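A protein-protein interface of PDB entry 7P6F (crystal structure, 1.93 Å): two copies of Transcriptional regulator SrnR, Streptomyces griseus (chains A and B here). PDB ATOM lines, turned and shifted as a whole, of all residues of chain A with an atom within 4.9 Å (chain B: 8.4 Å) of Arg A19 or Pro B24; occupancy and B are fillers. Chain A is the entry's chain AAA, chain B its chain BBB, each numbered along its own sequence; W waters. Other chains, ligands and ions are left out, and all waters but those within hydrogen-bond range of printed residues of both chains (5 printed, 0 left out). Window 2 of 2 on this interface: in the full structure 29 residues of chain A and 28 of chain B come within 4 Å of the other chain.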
ATOM      1  N   ALA A  15      13.840  24.873  17.792  1.00  0.00           N
ATOM      2  CA  ALA A  15      15.273  24.498  17.897  1.00  0.00           C
ATOM      3  C   ALA A  15      15.543  23.840  19.253  1.00  0.00           C
ATOM      4  O   ALA A  15      16.191  22.772  19.248  1.00  0.00           O
ATOM      5  CB  ALA A  15      16.209  25.649  17.662  1.00  0.00           C
ATOM      6  N   SER A  16      15.103  24.422  20.372  1.00  0.00           N
ATOM      7  CA  SER A  16      15.463  23.857  21.699  1.00  0.00           C
ATOM      8  C   SER A  16      14.747  22.519  21.886  1.00  0.00           C
ATOM      9  O   SER A  16      15.346  21.610  22.476  1.00  0.00           O
ATOM     10  CB  SER A  16      15.263  24.866  22.827  1.00  0.00           C
ATOM     11  OG  SER A  16      13.890  25.079  22.991  1.00  0.00           O
ATOM     12  N   ALA A  17      13.547  22.344  21.338  1.00  0.00           N
ATOM     13  CA  ALA A  17      12.785  21.077  21.399  1.00  0.00           C
ATOM     14  C   ALA A  17      13.524  19.980  20.625  1.00  0.00           C
ATOM     15  O   ALA A  17      13.712  18.874  21.171  1.00  0.00           O
ATOM     16  CB  ALA A  17      11.375  21.254  20.863  1.00  0.00           C
ATOM     17  N   PHE A  18      14.009  20.269  19.423  1.00  0.00           N
ATOM     18  CA  PHE A  18      14.792  19.309  18.597  1.00  0.00           C
ATOM     19  C   PHE A  18      16.118  18.949  19.284  1.00  0.00           C
ATOM     20  O   PHE A  18      16.498  17.765  19.246  1.00  0.00           O
ATOM     21  CB  PHE A  18      14.950  19.788  17.142  1.00  0.00           C
ATOM     22  CG  PHE A  18      13.734  19.437  16.312  1.00  0.00           C
ATOM     23  CD1 PHE A  18      13.594  18.169  15.802  1.00  0.00           C
ATOM     24  CD2 PHE A  18      12.746  20.365  16.023  1.00  0.00           C
ATOM     25  CE1 PHE A  18      12.471  17.814  15.063  1.00  0.00           C
ATOM     26  CE2 PHE A  18      11.614  19.989  15.309  1.00  0.00           C
ATOM     27  CZ  PHE A  18      11.482  18.728  14.802  1.00  0.00           C
ATOM     28  N   ARG A  19      16.821  19.907  19.904  1.00  0.00           N
ATOM     29  CA  ARG A  19      18.071  19.594  20.637  1.00  0.00           C
ATOM     30  C   ARG A  19      17.749  18.691  21.840  1.00  0.00           C
ATOM     31  O   ARG A  19      18.527  17.752  22.129  1.00  0.00           O
ATOM     32  CB  ARG A  19      18.806  20.874  21.011  1.00  0.00           C
ATOM     33  CG  ARG A  19      19.321  21.673  19.811  1.00  0.00           C
ATOM     34  CD  ARG A  19      20.404  20.924  19.028  1.00  0.00           C
ATOM     35  NE  ARG A  19      20.986  21.748  18.007  1.00  0.00           N
ATOM     36  CZ  ARG A  19      21.825  21.299  17.081  1.00  0.00           C
ATOM     37  NH1 ARG A  19      22.265  20.054  17.122  1.00  0.00           N
ATOM     38  NH2 ARG A  19      22.240  22.101  16.128  1.00  0.00           N
ATOM     39  N   ALA A  20      16.581  18.867  22.444  1.00  0.00           N
ATOM     40  CA  ALA A  20      16.188  18.109  23.648  1.00  0.00           C
ATOM     41  C   ALA A  20      15.904  16.654  23.254  1.00  0.00           C
ATOM     42  O   ALA A  20      16.406  15.740  23.957  1.00  0.00           O
ATOM     43  CB  ALA A  20      15.020  18.786  24.345  1.00  0.00           C
ATOM     44  N   VAL A  21      15.139  16.422  22.183  1.00  0.00           N
ATOM     45  CA  VAL A  21      14.730  15.058  21.781  1.00  0.00           C
ATOM     46  C   VAL A  21      15.819  14.395  20.937  1.00  0.00           C
ATOM     47  O   VAL A  21      15.651  13.210  20.600  1.00  0.00           O
ATOM     48  CB  VAL A  21      13.347  15.036  21.114  1.00  0.00           C
ATOM     49  CG1 VAL A  21      12.266  15.580  22.053  1.00  0.00           C
ATOM     50  CG2 VAL A  21      13.295  15.734  19.767  1.00  0.00           C
ATOM     51  N   ALA A  22      16.928  15.071  20.648  1.00  0.00           N
ATOM     52  CA  ALA A  22      18.075  14.473  19.939  1.00  0.00           C
ATOM     53  C   ALA A  22      18.668  13.348  20.787  1.00  0.00           C
ATOM     54  O   ALA A  22      19.285  12.439  20.216  1.00  0.00           O
ATOM     55  CB  ALA A  22      19.132  15.522  19.656  1.00  0.00           C
ATOM     56  N   ASP A  23      18.461  13.397  22.096  1.00  0.00           N
ATOM     57  CA  ASP A  23      19.198  12.481  23.015  1.00  0.00           C
ATOM     58  C   ASP A  23      18.306  11.295  23.410  1.00  0.00           C
ATOM     59  O   ASP A  23      17.169  11.529  23.777  1.00  0.00           O
ATOM     60  CB  ASP A  23      19.700  13.240  24.250  1.00  0.00           C
ATOM     61  CG  ASP A  23      20.344  12.313  25.270  1.00  0.00           C
ATOM     62  OD1 ASP A  23      19.598  11.689  26.063  1.00  0.00           O
ATOM     63  OD2 ASP A  23      21.594  12.209  25.238  1.00  0.00           O
ATOM     64  N   ARG A  26      16.834  11.294  26.968  1.00  0.00           N
ATOM     65  CA  ARG A  26      15.764  12.270  27.181  1.00  0.00           C
ATOM     66  C   ARG A  26      14.496  11.730  26.511  1.00  0.00           C
ATOM     67  O   ARG A  26      13.374  12.016  27.020  1.00  0.00           O
ATOM     68  CB  ARG A  26      16.173  13.650  26.668  1.00  0.00           C
ATOM     69  CG  ARG A  26      17.263  14.231  27.551  1.00  0.00           C
ATOM     70  CD  ARG A  26      17.490  15.680  27.255  1.00  0.00           C
ATOM     71  NE  ARG A  26      18.107  15.997  25.980  1.00  0.00           N
ATOM     72  CZ  ARG A  26      19.413  16.223  25.775  1.00  0.00           C
ATOM     73  NH1 ARG A  26      20.288  16.028  26.734  1.00  0.00           N
ATOM     74  NH2 ARG A  26      19.845  16.645  24.601  1.00  0.00           N
ATOM     75  N   PHE B  18      16.823  11.170  14.736  1.00  0.00           N
ATOM     76  CA  PHE B  18      16.743  12.250  15.760  1.00  0.00           C
ATOM     77  C   PHE B  18      18.033  13.084  15.786  1.00  0.00           C
ATOM     78  O   PHE B  18      17.945  14.321  15.883  1.00  0.00           O
ATOM     79  CB  PHE B  18      16.316  11.694  17.123  1.00  0.00           C
ATOM     80  CG  PHE B  18      14.807  11.624  17.264  1.00  0.00           C
ATOM     81  CD1 PHE B  18      14.065  12.779  17.494  1.00  0.00           C
ATOM     82  CD2 PHE B  18      14.138  10.413  17.260  1.00  0.00           C
ATOM     83  CE1 PHE B  18      12.682  12.725  17.619  1.00  0.00           C
ATOM     84  CE2 PHE B  18      12.753  10.362  17.412  1.00  0.00           C
ATOM     85  CZ  PHE B  18      12.027  11.522  17.559  1.00  0.00           C
ATOM     86  N   ARG B  19      19.194  12.464  15.579  1.00  0.00           N
ATOM     87  CA  ARG B  19      20.476  13.202  15.498  1.00  0.00           C
ATOM     88  C   ARG B  19      20.538  13.978  14.174  1.00  0.00           C
ATOM     89  O   ARG B  19      21.194  15.001  14.157  1.00  0.00           O
ATOM     90  CB  ARG B  19      21.664  12.256  15.700  1.00  0.00           C
ATOM     91  CG  ARG B  19      21.935  11.921  17.167  1.00  0.00           C
ATOM     92  CD  ARG B  19      23.214  11.115  17.352  1.00  0.00           C
ATOM     93  NE  ARG B  19      23.036   9.808  16.730  1.00  0.00           N
ATOM     94  CZ  ARG B  19      22.690   8.656  17.334  1.00  0.00           C
ATOM     95  NH1 ARG B  19      22.463   8.571  18.648  1.00  0.00           N
ATOM     96  NH2 ARG B  19      22.550   7.609  16.547  1.00  0.00           N
ATOM     97  N   ALA B  20      19.895  13.495  13.104  1.00  0.00           N
ATOM     98  CA  ALA B  20      19.845  14.222  11.806  1.00  0.00           C
ATOM     99  C   ALA B  20      18.917  15.442  11.929  1.00  0.00           C
ATOM    100  O   ALA B  20      19.324  16.547  11.516  1.00  0.00           O
ATOM    101  CB  ALA B  20      19.413  13.281  10.693  1.00  0.00           C
ATOM    102  N   VAL B  21      17.713  15.290  12.484  1.00  0.00           N
ATOM    103  CA  VAL B  21      16.748  16.433  12.587  1.00  0.00           C
ATOM    104  C   VAL B  21      17.090  17.339  13.779  1.00  0.00           C
ATOM    105  O   VAL B  21      16.428  18.374  13.915  1.00  0.00           O
ATOM    106  CB  VAL B  21      15.267  15.991  12.576  1.00  0.00           C
ATOM    107  CG1 VAL B  21      14.953  15.291  11.253  1.00  0.00           C
ATOM    108  CG2 VAL B  21      14.887  15.183  13.794  1.00  0.00           C
ATOM    109  N   ALA B  22      18.162  17.048  14.534  1.00  0.00           N
ATOM    110  CA  ALA B  22      18.615  17.899  15.647  1.00  0.00           C
ATOM    111  C   ALA B  22      19.026  19.288  15.125  1.00  0.00           C
ATOM    112  O   ALA B  22      18.957  20.257  15.921  1.00  0.00           O
ATOM    113  CB  ALA B  22      19.748  17.262  16.396  1.00  0.00           C
ATOM    114  N   ASP B  23      19.515  19.364  13.886  1.00  0.00           N
ATOM    115  CA  ASP B  23      20.201  20.548  13.336  1.00  0.00           C
ATOM    116  C   ASP B  23      19.215  21.374  12.519  1.00  0.00           C
ATOM    117  O   ASP B  23      18.528  20.847  11.677  1.00  0.00           O
ATOM    118  CB  ASP B  23      21.405  20.130  12.500  1.00  0.00           C
ATOM    119  CG  ASP B  23      22.100  21.312  11.857  1.00  0.00           C
ATOM    120  OD1 ASP B  23      21.666  21.716  10.788  1.00  0.00           O
ATOM    121  OD2 ASP B  23      23.086  21.768  12.394  1.00  0.00           O
ATOM    122  N   PRO B  24      19.167  22.704  12.687  1.00  0.00           N
ATOM    123  CA  PRO B  24      18.237  23.549  11.942  1.00  0.00           C
ATOM    124  C   PRO B  24      18.512  23.610  10.434  1.00  0.00           C
ATOM    125  O   PRO B  24      17.533  23.595   9.666  1.00  0.00           O
ATOM    126  CB  PRO B  24      18.375  24.943  12.602  1.00  0.00           C
ATOM    127  CG  PRO B  24      19.773  24.928  13.177  1.00  0.00           C
ATOM    128  CD  PRO B  24      20.017  23.487  13.601  1.00  0.00           C
ATOM    129  N   THR B  25      19.774  23.551  10.017  1.00  0.00           N
ATOM    130  CA  THR B  25      20.101  23.496   8.581  1.00  0.00           C
ATOM    131  C   THR B  25      19.519  22.211   7.978  1.00  0.00           C
ATOM    132  O   THR B  25      18.860  22.270   6.906  1.00  0.00           O
ATOM    133  CB  THR B  25      21.597  23.654   8.356  1.00  0.00           C
ATOM    134  OG1 THR B  25      21.905  24.910   8.941  1.00  0.00           O
ATOM    135  CG2 THR B  25      21.949  23.655   6.895  1.00  0.00           C
ATOM    136  N   ARG B  26      19.699  21.061   8.631  1.00  0.00           N
ATOM    137  CA  ARG B  26      19.124  19.814   8.107  1.00  0.00           C
ATOM    138  C   ARG B  26      17.591  19.861   8.083  1.00  0.00           C
ATOM    139  O   ARG B  26      17.022  19.375   7.101  1.00  0.00           O
ATOM    140  CB  ARG B  26      19.719  18.681   8.932  1.00  0.00           C
ATOM    141  CG  ARG B  26      21.222  18.610   8.675  1.00  0.00           C
ATOM    142  CD  ARG B  26      21.786  17.285   9.098  1.00  0.00           C
ATOM    143  NE  ARG B  26      21.820  17.100  10.540  1.00  0.00           N
ATOM    144  CZ  ARG B  26      22.904  17.224  11.300  1.00  0.00           C
ATOM    145  NH1 ARG B  26      24.026  17.726  10.824  1.00  0.00           N
ATOM    146  NH2 ARG B  26      22.838  16.942  12.570  1.00  0.00           N
ATOM    147  N   ARG B  27      16.924  20.417   9.091  1.00  0.00           N
ATOM    148  CA  ARG B  27      15.454  20.513   9.011  1.00  0.00           C
ATOM    149  C   ARG B  27      15.057  21.402   7.808  1.00  0.00           C
ATOM    150  O   ARG B  27      14.109  21.044   7.087  1.00  0.00           O
ATOM    151  CB  ARG B  27      14.918  21.083  10.324  1.00  0.00           C
ATOM    152  CG  ARG B  27      15.060  20.123  11.508  1.00  0.00           C
ATOM    153  CD  ARG B  27      14.126  20.557  12.645  1.00  0.00           C
ATOM    154  NE  ARG B  27      14.458  21.849  13.238  1.00  0.00           N
ATOM    155  CZ  ARG B  27      15.480  22.106  14.052  1.00  0.00           C
ATOM    156  NH1 ARG B  27      16.310  21.151  14.407  1.00  0.00           N
ATOM    157  NH2 ARG B  27      15.668  23.311  14.551  1.00  0.00           N
ATOM    158  N   GLN B  28      15.766  22.506   7.582  1.00  0.00           N
ATOM    159  CA  GLN B  28      15.424  23.429   6.469  1.00  0.00           C
ATOM    160  C   GLN B  28      15.656  22.702   5.153  1.00  0.00           C
ATOM    161  O   GLN B  28      14.816  22.850   4.219  1.00  0.00           O
ATOM    162  CB  GLN B  28      16.172  24.745   6.558  1.00  0.00           C
ATOM    163  CG  GLN B  28      15.673  25.785   5.546  1.00  0.00           C
ATOM    164  CD  GLN B  28      14.221  26.147   5.769  1.00  0.00           C
ATOM    165  OE1 GLN B  28      13.925  26.845   6.717  1.00  0.00           O
ATOM    166  NE2 GLN B  28      13.291  25.628   4.976  1.00  0.00           N
ATOM    167  N   ILE B  29      16.746  21.952   5.031  1.00  0.00           N
ATOM    168  CA  ILE B  29      16.956  21.180   3.776  1.00  0.00           C
ATOM    169  C   ILE B  29      15.751  20.262   3.527  1.00  0.00           C
ATOM    170  O   ILE B  29      15.316  20.171   2.401  1.00  0.00           O
ATOM    171  CB  ILE B  29      18.276  20.390   3.799  1.00  0.00           C
ATOM    172  CG1 ILE B  29      19.459  21.352   3.705  1.00  0.00           C
ATOM    173  CG2 ILE B  29      18.271  19.325   2.699  1.00  0.00           C
ATOM    174  CD1 ILE B  29      20.760  20.764   4.178  1.00  0.00           C
ATOM    175  N   LEU B  30      15.308  19.516   4.554  1.00  0.00           N
ATOM    176  CA  LEU B  30      14.174  18.570   4.403  1.00  0.00           C
ATOM    177  C   LEU B  30      12.920  19.320   3.981  1.00  0.00           C
ATOM    178  O   LEU B  30      12.162  18.846   3.073  1.00  0.00           O
ATOM    179  CB  LEU B  30      13.971  17.813   5.725  1.00  0.00           C
ATOM    180  CG  LEU B  30      15.083  16.852   6.082  1.00  0.00           C
ATOM    181  CD1 LEU B  30      14.874  16.256   7.459  1.00  0.00           C
ATOM    182  CD2 LEU B  30      15.156  15.703   5.097  1.00  0.00           C
ATOM    183  N   GLU B  31      12.706  20.472   4.568  1.00  0.00           N
ATOM    184  CA  GLU B  31      11.557  21.319   4.177  1.00  0.00           C
ATOM    185  C   GLU B  31      11.698  21.783   2.717  1.00  0.00           C
ATOM    186  O   GLU B  31      10.714  21.685   1.947  1.00  0.00           O
ATOM    187  CB  GLU B  31      11.385  22.504   5.129  1.00  0.00           C
ATOM    188  CG  GLU B  31      10.763  22.139   6.481  1.00  0.00           C
ATOM    189  CD  GLU B  31      10.330  23.386   7.230  1.00  0.00           C
ATOM    190  OE1 GLU B  31       9.535  24.109   6.667  1.00  0.00           O
ATOM    191  OE2 GLU B  31      10.869  23.675   8.274  1.00  0.00           O
ATOM    192  N   PHE B  47      21.594  28.432   1.201  1.00  0.00           N
ATOM    193  CA  PHE B  47      22.183  28.604   2.554  1.00  0.00           C
ATOM    194  C   PHE B  47      23.470  29.419   2.486  1.00  0.00           C
ATOM    195  O   PHE B  47      24.350  29.071   1.736  1.00  0.00           O
ATOM    196  CB  PHE B  47      22.450  27.234   3.203  1.00  0.00           C
ATOM    197  CG  PHE B  47      21.200  26.444   3.451  1.00  0.00           C
ATOM    198  CD1 PHE B  47      20.426  26.657   4.586  1.00  0.00           C
ATOM    199  CD2 PHE B  47      20.792  25.505   2.532  1.00  0.00           C
ATOM    200  CE1 PHE B  47      19.250  25.960   4.778  1.00  0.00           C
ATOM    201  CE2 PHE B  47      19.605  24.809   2.710  1.00  0.00           C
ATOM    202  CZ  PHE B  47      18.837  25.025   3.834  1.00  0.00           C
ATOM    203  N   HIS B  57      26.132  18.127   5.854  1.00  0.00           N
ATOM    204  CA  HIS B  57      24.705  18.051   6.285  1.00  0.00           C
ATOM    205  C   HIS B  57      23.973  17.043   5.414  1.00  0.00           C
ATOM    206  O   HIS B  57      23.231  16.193   5.924  1.00  0.00           O
ATOM    207  CB  HIS B  57      24.053  19.424   6.265  1.00  0.00           C
ATOM    208  CG  HIS B  57      24.471  20.313   7.381  1.00  0.00           C
ATOM    209  ND1 HIS B  57      24.417  19.904   8.685  1.00  0.00           N
ATOM    210  CD2 HIS B  57      24.986  21.576   7.391  1.00  0.00           C
ATOM    211  CE1 HIS B  57      24.875  20.883   9.466  1.00  0.00           C
ATOM    212  NE2 HIS B  57      25.204  21.920   8.704  1.00  0.00           N
HETATM  213  O   HOH W   1      17.867  22.840  16.594  1.00  0.00           O
HETATM  214  O   HOH W   2      15.963  15.807  17.235  1.00  0.00           O
HETATM  215  O   HOH W   3      24.286  20.667  14.412  1.00  0.00           O
HETATM  216  O   HOH W   4      24.197  18.053  15.262  1.00  0.00           O
HETATM  217  O   HOH W   5      19.373   9.768  19.082  1.00  0.00           O
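Water W3 lies within hydrogen-bond range of the side-chain carboxylate (OD2) of Asp B23 (2.6 Å) and the guanidinium group (NH2) of Arg A19 (3.0 Å). Water W2 bridges O of Phe B18 (2.8 Å) and O of Phe A18 (2.9 Å). Water W1 lies within hydrogen-bond range of the backbone carbonyl oxygen (O) of Ala B22 (2.9 Å), the guanidinium group (NH2) of Arg B27 (3.0 Å) and the backbone carbonyl oxygen (O) of Ala A15 (3.1 Å). Water W5 bridges O of Ala A22 (2.9 Å) and NH1 of Arg B19 (3.3 Å). Water W4 bridges NH2 of Arg B26 (3.2 Å) and NH1 of Arg A19 (3.3 Å).
The guanidinium group (NH2) of Arg A26 is in hydrogen-bond range of the backbone carbonyl oxygen (O) of Arg A19 (3.0 Å). The backbone carbonyl oxygen of Val B21 is in hydrogen-bond range of the guanidinium group of Arg B27 (2.8 Å). The side-chain carboxylate of Asp B23 is in hydrogen-bond range of the backbone NH of Thr B25 (2.7 Å). The backbone carbonyl oxygen (O) of Ala B22 is in hydrogen-bond range of the guanidinium group (NH1) of Arg B27 (3.2 Å). The side-chain carboxylate (OD1) of Asp B23 is in hydrogen-bond range of the backbone NH (N) of Arg B26 (3.0 Å).
Ala A15 touches Arg B27. O of Val B21 touches CD1 of Phe A18, 3.4 Å away. CB of Phe A18 touches NH1 of Arg B27 (3.3 Å). Pro B24 touches Arg A19 (CD to NH2, 3.6 Å). Phe B18 touches Val A21 (CD1 to O, 3.5 Å). Ala A22 touches Ala B22.
Arg A19 touches just these residues of chain B: Ala B22 (3.3 Å), Asp B23 (3.8 Å) and Pro B24 (3.6 Å). Of chain A, only Arg A19 comes within 4 Å of Pro B24. Printed residues of chain A within 4 Å of Asp B23: Arg A19. Of the printed residues of chain B, Val A21 touches Phe B18. Printed residues of chain A within 4 Å of Val B21: Phe A18 (3.4 Å). Of the printed residues of chain A, Ala B22 touches Arg A19 and Ala A22. Of the printed residues of chain B, Ala A15 touches Arg B27. Ala A17 touches none of the printed residues of chain B. The nearest residue of chain B that does not touch Arg A19 is Arg B26 (5.5 Å). The nearest printed residue of chain A that does not touch Pro B24 is Ala A15 (5.5 Å).
The backbone carbonyl oxygen (O) of Ala B22 sits close to the guanidinium group (NE) of Arg A19 (3.3 Å). The guanidinium group (NH2) of Arg A19 is in salt-bridge range of the side-chain carboxylate (OD2) of Asp B23 (3.8 Å).
Phe A18 touches Val B21, and with the chains exchanged Val A21 touches Phe B18. Arg A19 touches Ala B22, but with the chains exchanged Ala A22 does not touch Arg B19 (4.1 Å). Arg A19 touches Asp B23, but with the chains exchanged Asp A23 does not touch Arg B19 (6.2 Å). Ala B22 touches its own counterpart, Ala A22. Of the 8 pairs that touch across the chains among the printed residues, 3 have their exchanged pair printed and touching as well.
Hydrophobic or aromatic side chains of chain A within 4 Å of the printed part of chain B: Ala A15, Phe A18, Val A21 and Ala A22. Among the printed residues, 8 pairs touch across the chains.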
